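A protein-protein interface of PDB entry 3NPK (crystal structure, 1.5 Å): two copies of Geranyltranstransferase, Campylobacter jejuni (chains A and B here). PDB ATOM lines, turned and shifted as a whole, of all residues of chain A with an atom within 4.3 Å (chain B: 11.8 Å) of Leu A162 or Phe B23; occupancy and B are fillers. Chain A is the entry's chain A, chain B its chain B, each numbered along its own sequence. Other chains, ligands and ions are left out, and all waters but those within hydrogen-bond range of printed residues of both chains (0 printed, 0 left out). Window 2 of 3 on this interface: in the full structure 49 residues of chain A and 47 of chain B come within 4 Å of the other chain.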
ATOM      1  N   ILE A 153     -15.735   4.473  -2.790  1.00  0.00           N
ATOM      2  CA  ILE A 153     -15.891   5.908  -2.591  1.00  0.00           C
ATOM      3  C   ILE A 153     -15.385   6.322  -1.203  1.00  0.00           C
ATOM      4  O   ILE A 153     -14.646   7.305  -1.063  1.00  0.00           O
ATOM      5  CB  ILE A 153     -17.353   6.315  -2.814  1.00  0.00           C
ATOM      6  CG1 ILE A 153     -17.651   6.249  -4.314  1.00  0.00           C
ATOM      7  CG2 ILE A 153     -17.648   7.724  -2.258  1.00  0.00           C
ATOM      8  CD1 ILE A 153     -19.129   6.423  -4.678  1.00  0.00           C
ATOM      9  N   PHE A 157     -12.251   8.939  -1.016  1.00  0.00           N
ATOM     10  CA  PHE A 157     -12.550  10.306  -0.589  1.00  0.00           C
ATOM     11  C   PHE A 157     -12.331  10.535   0.907  1.00  0.00           C
ATOM     12  O   PHE A 157     -12.693  11.582   1.442  1.00  0.00           O
ATOM     13  CB  PHE A 157     -13.977  10.715  -1.013  1.00  0.00           C
ATOM     14  CG  PHE A 157     -14.155  10.817  -2.506  1.00  0.00           C
ATOM     15  CD1 PHE A 157     -13.814  11.988  -3.175  1.00  0.00           C
ATOM     16  CD2 PHE A 157     -14.667   9.753  -3.245  1.00  0.00           C
ATOM     17  CE1 PHE A 157     -13.972  12.101  -4.555  1.00  0.00           C
ATOM     18  CE2 PHE A 157     -14.839   9.864  -4.616  1.00  0.00           C
ATOM     19  CZ  PHE A 157     -14.486  11.033  -5.282  1.00  0.00           C
ATOM     20  N   LYS A 160     -10.610  13.752   1.221  1.00  0.00           N
ATOM     21  CA  LYS A 160     -11.081  14.759   0.273  1.00  0.00           C
ATOM     22  C   LYS A 160     -12.438  15.303   0.708  1.00  0.00           C
ATOM     23  O   LYS A 160     -13.183  14.642   1.435  1.00  0.00           O
ATOM     24  CB  LYS A 160     -11.163  14.150  -1.136  1.00  0.00           C
ATOM     25  CG  LYS A 160      -9.823  13.616  -1.636  1.00  0.00           C
ATOM     26  CD  LYS A 160      -9.967  12.918  -2.983  1.00  0.00           C
ATOM     27  CE  LYS A 160      -8.645  12.341  -3.463  1.00  0.00           C
ATOM     28  NZ  LYS A 160      -8.217  11.194  -2.615  1.00  0.00           N
ATOM     29  N   ARG A 161     -12.761  16.508   0.261  1.00  0.00           N
ATOM     30  CA  ARG A 161     -14.013  17.141   0.664  1.00  0.00           C
ATOM     31  C   ARG A 161     -15.194  16.637  -0.163  1.00  0.00           C
ATOM     32  O   ARG A 161     -15.167  16.680  -1.406  1.00  0.00           O
ATOM     33  CB  ARG A 161     -13.915  18.663   0.526  1.00  0.00           C
ATOM     34  CG  ARG A 161     -15.201  19.374   0.935  1.00  0.00           C
ATOM     35  CD  ARG A 161     -15.102  20.883   0.688  1.00  0.00           C
ATOM     36  NE  ARG A 161     -14.918  21.192  -0.732  1.00  0.00           N
ATOM     37  CZ  ARG A 161     -15.900  21.170  -1.625  1.00  0.00           C
ATOM     38  NH1 ARG A 161     -17.129  20.843  -1.247  1.00  0.00           N
ATOM     39  NH2 ARG A 161     -15.654  21.469  -2.895  1.00  0.00           N
ATOM     40  N   LEU A 162     -16.226  16.166   0.536  1.00  0.00           N
ATOM     41  CA  LEU A 162     -17.470  15.724  -0.085  1.00  0.00           C
ATOM     42  C   LEU A 162     -18.578  16.718   0.199  1.00  0.00           C
ATOM     43  O   LEU A 162     -18.601  17.350   1.261  1.00  0.00           O
ATOM     44  CB  LEU A 162     -17.898  14.368   0.482  1.00  0.00           C
ATOM     45  CG  LEU A 162     -16.999  13.191   0.122  1.00  0.00           C
ATOM     46  CD1 LEU A 162     -17.541  11.892   0.682  1.00  0.00           C
ATOM     47  CD2 LEU A 162     -16.803  13.114  -1.397  1.00  0.00           C
ATOM     48  N   SER A 163     -19.505  16.829  -0.745  1.00  0.00           N
ATOM     49  CA  SER A 163     -20.730  17.578  -0.541  1.00  0.00           C
ATOM     50  C   SER A 163     -21.692  16.704   0.250  1.00  0.00           C
ATOM     51  O   SER A 163     -21.471  15.499   0.406  1.00  0.00           O
ATOM     52  CB  SER A 163     -21.364  17.910  -1.888  1.00  0.00           C
ATOM     53  OG  SER A 163     -21.869  16.720  -2.472  1.00  0.00           O
ATOM     54  N   LEU A 164     -22.776  17.305   0.719  1.00  0.00           N
ATOM     55  CA  LEU A 164     -23.813  16.567   1.436  1.00  0.00           C
ATOM     56  C   LEU A 164     -24.389  15.466   0.554  1.00  0.00           C
ATOM     57  O   LEU A 164     -24.529  14.320   0.986  1.00  0.00           O
ATOM     58  CB  LEU A 164     -24.936  17.524   1.844  1.00  0.00           C
ATOM     59  CG  LEU A 164     -25.719  17.287   3.141  1.00  0.00           C
ATOM     60  CD1 LEU A 164     -27.173  17.783   3.035  1.00  0.00           C
ATOM     61  CD2 LEU A 164     -25.657  15.883   3.638  1.00  0.00           C
ATOM     62  N   GLU A 166     -23.035  13.950  -1.941  1.00  0.00           N
ATOM     63  CA  GLU A 166     -22.012  12.928  -2.136  1.00  0.00           C
ATOM     64  C   GLU A 166     -21.857  12.037  -0.907  1.00  0.00           C
ATOM     65  O   GLU A 166     -21.726  10.811  -1.022  1.00  0.00           O
ATOM     66  CB  GLU A 166     -20.674  13.578  -2.489  1.00  0.00           C
ATOM     67  CG  GLU A 166     -20.667  14.063  -3.921  1.00  0.00           C
ATOM     68  CD  GLU A 166     -19.487  14.952  -4.254  1.00  0.00           C
ATOM     69  OE1 GLU A 166     -18.849  15.502  -3.327  1.00  0.00           O
ATOM     70  OE2 GLU A 166     -19.208  15.099  -5.460  1.00  0.00           O
ATOM     71  N   PHE A 169     -24.750   9.728  -0.808  1.00  0.00           N
ATOM     72  CA  PHE A 169     -24.555   8.669  -1.808  1.00  0.00           C
ATOM     73  C   PHE A 169     -23.618   7.597  -1.252  1.00  0.00           C
ATOM     74  O   PHE A 169     -23.890   6.388  -1.334  1.00  0.00           O
ATOM     75  CB  PHE A 169     -23.983   9.280  -3.103  1.00  0.00           C
ATOM     76  CG  PHE A 169     -23.847   8.297  -4.253  1.00  0.00           C
ATOM     77  CD1 PHE A 169     -22.785   7.391  -4.292  1.00  0.00           C
ATOM     78  CD2 PHE A 169     -24.770   8.290  -5.308  1.00  0.00           C
ATOM     79  CE1 PHE A 169     -22.647   6.497  -5.343  1.00  0.00           C
ATOM     80  CE2 PHE A 169     -24.624   7.400  -6.366  1.00  0.00           C
ATOM     81  CZ  PHE A 169     -23.560   6.502  -6.381  1.00  0.00           C
ATOM     82  N   LEU A 170     -22.505   8.057  -0.691  1.00  0.00           N
ATOM     83  CA  LEU A 170     -21.505   7.157  -0.111  1.00  0.00           C
ATOM     84  C   LEU A 170     -22.162   6.194   0.873  1.00  0.00           C
ATOM     85  O   LEU A 170     -22.045   4.980   0.740  1.00  0.00           O
ATOM     86  CB  LEU A 170     -20.410   7.998   0.570  1.00  0.00           C
ATOM     87  CG  LEU A 170     -19.196   7.316   1.202  1.00  0.00           C
ATOM     88  CD1 LEU A 170     -18.175   8.407   1.518  1.00  0.00           C
ATOM     89  CD2 LEU A 170     -19.538   6.516   2.468  1.00  0.00           C
ATOM     90  N   ASN A 238     -15.013  13.847   6.537  1.00  0.00           N
ATOM     91  CA  ASN A 238     -16.374  14.125   6.079  1.00  0.00           C
ATOM     92  C   ASN A 238     -17.416  13.594   7.045  1.00  0.00           C
ATOM     93  O   ASN A 238     -17.493  12.393   7.285  1.00  0.00           O
ATOM     94  CB  ASN A 238     -16.620  13.494   4.708  1.00  0.00           C
ATOM     95  CG  ASN A 238     -15.695  14.045   3.636  1.00  0.00           C
ATOM     96  OD1 ASN A 238     -15.778  15.221   3.275  1.00  0.00           O
ATOM     97  ND2 ASN A 238     -14.811  13.196   3.126  1.00  0.00           N
ATOM     98  N   LEU A 243     -20.927  19.121   7.991  1.00  0.00           N
ATOM     99  CA  LEU A 243     -21.637  19.747   6.885  1.00  0.00           C
ATOM    100  C   LEU A 243     -22.877  20.494   7.344  1.00  0.00           C
ATOM    101  O   LEU A 243     -23.153  21.601   6.874  1.00  0.00           O
ATOM    102  CB  LEU A 243     -22.038  18.698   5.847  1.00  0.00           C
ATOM    103  CG  LEU A 243     -20.904  18.065   5.046  1.00  0.00           C
ATOM    104  CD1 LEU A 243     -21.442  17.009   4.103  1.00  0.00           C
ATOM    105  CD2 LEU A 243     -20.169  19.142   4.269  1.00  0.00           C
ATOM    106  N   LYS B  19     -20.451  -1.820 -14.789  1.00  0.00           N
ATOM    107  CA  LYS B  19     -20.251  -0.429 -14.426  1.00  0.00           C
ATOM    108  C   LYS B  19     -21.387   0.079 -13.558  1.00  0.00           C
ATOM    109  O   LYS B  19     -22.490  -0.477 -13.553  1.00  0.00           O
ATOM    110  CB  LYS B  19     -20.134   0.425 -15.680  1.00  0.00           C
ATOM    111  CG  LYS B  19     -21.339   0.352 -16.578  1.00  0.00           C
ATOM    112  CD  LYS B  19     -21.096   1.152 -17.846  1.00  0.00           C
ATOM    113  CE  LYS B  19     -22.165   0.879 -18.880  1.00  0.00           C
ATOM    114  NZ  LYS B  19     -21.797   1.528 -20.167  1.00  0.00           N
ATOM    115  N   VAL B  20     -21.097   1.131 -12.812  1.00  0.00           N
ATOM    116  CA  VAL B  20     -22.099   1.774 -11.971  1.00  0.00           C
ATOM    117  C   VAL B  20     -21.930   3.270 -12.100  1.00  0.00           C
ATOM    118  O   VAL B  20     -20.810   3.775 -12.111  1.00  0.00           O
ATOM    119  CB  VAL B  20     -21.994   1.325 -10.472  1.00  0.00           C
ATOM    120  CG1 VAL B  20     -20.601   1.628  -9.886  1.00  0.00           C
ATOM    121  CG2 VAL B  20     -23.109   1.938  -9.627  1.00  0.00           C
ATOM    122  N   GLU B  21     -23.043   3.980 -12.214  1.00  0.00           N
ATOM    123  CA  GLU B  21     -22.976   5.434 -12.265  1.00  0.00           C
ATOM    124  C   GLU B  21     -22.607   5.991 -10.888  1.00  0.00           C
ATOM    125  O   GLU B  21     -23.291   5.732  -9.908  1.00  0.00           O
ATOM    126  CB  GLU B  21     -24.308   6.020 -12.745  1.00  0.00           C
ATOM    127  CG  GLU B  21     -24.229   7.527 -13.029  1.00  0.00           C
ATOM    128  CD  GLU B  21     -25.525   8.096 -13.588  1.00  0.00           C
ATOM    129  OE1 GLU B  21     -26.560   8.052 -12.882  1.00  0.00           O
ATOM    130  OE2 GLU B  21     -25.509   8.600 -14.732  1.00  0.00           O
ATOM    131  N   SER B  22     -21.519   6.749 -10.799  1.00  0.00           N
ATOM    132  CA  SER B  22     -21.154   7.369  -9.523  1.00  0.00           C
ATOM    133  C   SER B  22     -20.133   8.462  -9.762  1.00  0.00           C
ATOM    134  O   SER B  22     -19.635   8.615 -10.876  1.00  0.00           O
ATOM    135  CB  SER B  22     -20.566   6.345  -8.541  1.00  0.00           C
ATOM    136  OG  SER B  22     -19.169   6.206  -8.749  1.00  0.00           O
ATOM    137  N   PHE B  23     -19.810   9.203  -8.704  1.00  0.00           N
ATOM    138  CA  PHE B  23     -18.816  10.268  -8.795  1.00  0.00           C
ATOM    139  C   PHE B  23     -17.396   9.764  -8.517  1.00  0.00           C
ATOM    140  O   PHE B  23     -16.442  10.557  -8.436  1.00  0.00           O
ATOM    141  CB  PHE B  23     -19.179  11.451  -7.885  1.00  0.00           C
ATOM    142  CG  PHE B  23     -19.296  11.090  -6.428  1.00  0.00           C
ATOM    143  CD1 PHE B  23     -20.505  10.658  -5.893  1.00  0.00           C
ATOM    144  CD2 PHE B  23     -18.196  11.194  -5.585  1.00  0.00           C
ATOM    145  CE1 PHE B  23     -20.615  10.331  -4.554  1.00  0.00           C
ATOM    146  CE2 PHE B  23     -18.299  10.854  -4.238  1.00  0.00           C
ATOM    147  CZ  PHE B  23     -19.509  10.412  -3.723  1.00  0.00           C
ATOM    148  N   HIS B  24     -17.248   8.450  -8.370  1.00  0.00           N
ATOM    149  CA  HIS B  24     -15.905   7.874  -8.271  1.00  0.00           C
ATOM    150  C   HIS B  24     -15.189   8.128  -9.605  1.00  0.00           C
ATOM    151  O   HIS B  24     -15.707   7.772 -10.654  1.00  0.00           O
ATOM    152  CB  HIS B  24     -15.950   6.373  -7.979  1.00  0.00           C
ATOM    153  CG  HIS B  24     -14.630   5.827  -7.543  1.00  0.00           C
ATOM    154  ND1 HIS B  24     -13.527   5.806  -8.371  1.00  0.00           N
ATOM    155  CD2 HIS B  24     -14.223   5.315  -6.354  1.00  0.00           C
ATOM    156  CE1 HIS B  24     -12.504   5.283  -7.720  1.00  0.00           C
ATOM    157  NE2 HIS B  24     -12.897   4.979  -6.494  1.00  0.00           N
ATOM    158  N   PRO B  25     -13.995   8.735  -9.571  1.00  0.00           N
ATOM    159  CA  PRO B  25     -13.428   9.175 -10.851  1.00  0.00           C
ATOM    160  C   PRO B  25     -12.852   8.062 -11.727  1.00  0.00           C
ATOM    161  O   PRO B  25     -12.570   8.322 -12.893  1.00  0.00           O
ATOM    162  CB  PRO B  25     -12.310  10.130 -10.418  1.00  0.00           C
ATOM    163  CG  PRO B  25     -11.916   9.616  -9.057  1.00  0.00           C
ATOM    164  CD  PRO B  25     -13.237   9.277  -8.428  1.00  0.00           C
ATOM    165  N   PHE B  26     -12.652   6.856 -11.200  1.00  0.00           N
ATOM    166  CA  PHE B  26     -12.041   5.832 -12.044  1.00  0.00           C
ATOM    167  C   PHE B  26     -12.507   4.406 -11.826  1.00  0.00           C
ATOM    168  O   PHE B  26     -11.989   3.506 -12.461  1.00  0.00           O
ATOM    169  CB  PHE B  26     -10.511   5.877 -11.976  1.00  0.00           C
ATOM    170  CG  PHE B  26      -9.945   5.680 -10.596  1.00  0.00           C
ATOM    171  CD1 PHE B  26      -9.820   4.410 -10.047  1.00  0.00           C
ATOM    172  CD2 PHE B  26      -9.497   6.769  -9.860  1.00  0.00           C
ATOM    173  CE1 PHE B  26      -9.289   4.224  -8.775  1.00  0.00           C
ATOM    174  CE2 PHE B  26      -8.963   6.588  -8.582  1.00  0.00           C
ATOM    175  CZ  PHE B  26      -8.861   5.308  -8.043  1.00  0.00           C
ATOM    176  N   PHE B  27     -13.490   4.189 -10.957  1.00  0.00           N
ATOM    177  CA  PHE B  27     -13.851   2.800 -10.658  1.00  0.00           C
ATOM    178  C   PHE B  27     -14.323   2.022 -11.884  1.00  0.00           C
ATOM    179  O   PHE B  27     -13.951   0.863 -12.064  1.00  0.00           O
ATOM    180  CB  PHE B  27     -14.868   2.677  -9.529  1.00  0.00           C
ATOM    181  CG  PHE B  27     -14.841   1.327  -8.847  1.00  0.00           C
ATOM    182  CD1 PHE B  27     -13.819   1.008  -7.964  1.00  0.00           C
ATOM    183  CD2 PHE B  27     -15.831   0.389  -9.082  1.00  0.00           C
ATOM    184  CE1 PHE B  27     -13.780  -0.214  -7.324  1.00  0.00           C
ATOM    185  CE2 PHE B  27     -15.813  -0.852  -8.436  1.00  0.00           C
ATOM    186  CZ  PHE B  27     -14.781  -1.153  -7.552  1.00  0.00           C
ATOM    187  N   ASN B  28     -15.144   2.643 -12.726  1.00  0.00           N
ATOM    188  CA  ASN B  28     -15.593   1.943 -13.929  1.00  0.00           C
ATOM    189  C   ASN B  28     -14.445   1.624 -14.867  1.00  0.00           C
ATOM    190  O   ASN B  28     -14.401   0.563 -15.468  1.00  0.00           O
ATOM    191  CB  ASN B  28     -16.656   2.739 -14.674  1.00  0.00           C
ATOM    192  CG  ASN B  28     -17.957   2.796 -13.931  1.00  0.00           C
ATOM    193  OD1 ASN B  28     -18.280   1.906 -13.136  1.00  0.00           O
ATOM    194  ND2 ASN B  28     -18.727   3.839 -14.185  1.00  0.00           N
ATOM    195  N   GLU B  29     -13.524   2.563 -15.007  1.00  0.00           N
ATOM    196  CA  GLU B  29     -12.355   2.341 -15.829  1.00  0.00           C
ATOM    197  C   GLU B  29     -11.537   1.169 -15.280  1.00  0.00           C
ATOM    198  O   GLU B  29     -11.096   0.289 -16.032  1.00  0.00           O
ATOM    199  CB  GLU B  29     -11.516   3.621 -15.858  1.00  0.00           C
ATOM    200  CG  GLU B  29     -10.286   3.568 -16.726  1.00  0.00           C
ATOM    201  CD  GLU B  29      -9.438   4.826 -16.574  1.00  0.00           C
ATOM    202  OE1 GLU B  29      -8.624   4.912 -15.624  1.00  0.00           O
ATOM    203  OE2 GLU B  29      -9.589   5.737 -17.407  1.00  0.00           O
ATOM    204  N   LEU B  31     -12.619  -1.320 -13.399  1.00  0.00           N
ATOM    205  CA  LEU B  31     -13.392  -2.550 -13.556  1.00  0.00           C
ATOM    206  C   LEU B  31     -13.194  -3.123 -14.952  1.00  0.00           C
ATOM    207  O   LEU B  31     -13.068  -4.344 -15.138  1.00  0.00           O
ATOM    208  CB  LEU B  31     -14.885  -2.254 -13.373  1.00  0.00           C
ATOM    209  CG  LEU B  31     -15.531  -2.228 -11.983  1.00  0.00           C
ATOM    210  CD1 LEU B  31     -16.888  -1.528 -12.044  1.00  0.00           C
ATOM    211  CD2 LEU B  31     -15.665  -3.651 -11.392  1.00  0.00           C
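The backbone carbonyl oxygen (O) of Phe A157 lies within hydrogen-bond range of the side-chain amide nitrogen (ND2) of Asn A238 (3.2 Å). The backbone NH of Leu A162 lies within hydrogen-bond range of the side-chain amide oxygen of Asn A238. The backbone NH (N) of Ser A163 sits at hydrogen-bond distance from the side-chain carboxylate (OE1) of Glu A166. OG of Ser B22 sits at hydrogen-bond distance from N of His B24 (3.0 Å). N of Phe B26 is in hydrogen-bond range of ND1 of His B24 (3.1 Å). A ring nitrogen (ND1) of His B24 is in hydrogen-bond range of the backbone NH of Phe B27 (3.1 Å).
CG2 of Ile A153 touches CZ of Phe B23 (3.6 Å). His B24 touches Ile A153. Phe A157 touches Phe B23 (CE2 to CE2, 3.6 Å). Pro B25 touches Phe A157 (CD to CZ, 3.8 Å). CD2 of Leu A162 touches CE2 of Phe B23, at 3.9 Å. CZ of Phe B23 touches O of Glu A166 (3.5 Å). Phe A169 touches Glu B21 (CZ to O, 3.6 Å). CZ of Phe A169 touches CB of Ser B22 (3.7 Å). Phe B23 touches Phe A169.
Ile A153 touches two residues of chain B. Of chain B, only Phe B23 and Pro B25 come within 4 Å of Phe A157. Arg A161 touches none of the printed residues of chain B. Of chain B, only Phe B23 comes within 4 Å of Leu A162. Of chain B, only Glu B21, Ser B22 and Phe B23 come within 4 Å of Phe A169. No residue of chain B comes within 4 Å of Leu A170. No residue of chain B comes within 4 Å of Asn A238. Lys B19 touches none of the printed residues of chain A. Of the printed residues of chain A, Glu B21 touches Phe A169. Of the printed residues of chain A, Ser B22 touches Phe A169 (3.7 Å). Of chain A, only Ile A153, Phe A157, Leu A162, Glu A166 and Phe A169 come within 4 Å of Phe B23. Printed residues of chain A within 4 Å of His B24: Ile A153. Printed residues of chain A within 4 Å of Pro B25: Phe A157. The nearest residue of chain B that does not touch Leu A162 is His B24 (8.4 Å).
Printed residues of chain A that touch a printed residue of chain B: Ile A153, Phe A157, Leu A162, Glu A166 and Phe A169. Along chain B the printed residues that touch a printed residue of chain A span positions 21 to 25. Among the printed residues, 9 pairs touch across the chains. Among the printed residues, no Asp or Glu carboxylate lies within 4 Å of a Lys or Arg side-chain nitrogen of the other chain.
No position is printed for both chains. Of the 9 pairs that touch across the chains among the printed residues, none has its exchanged pair printed and touching as well.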
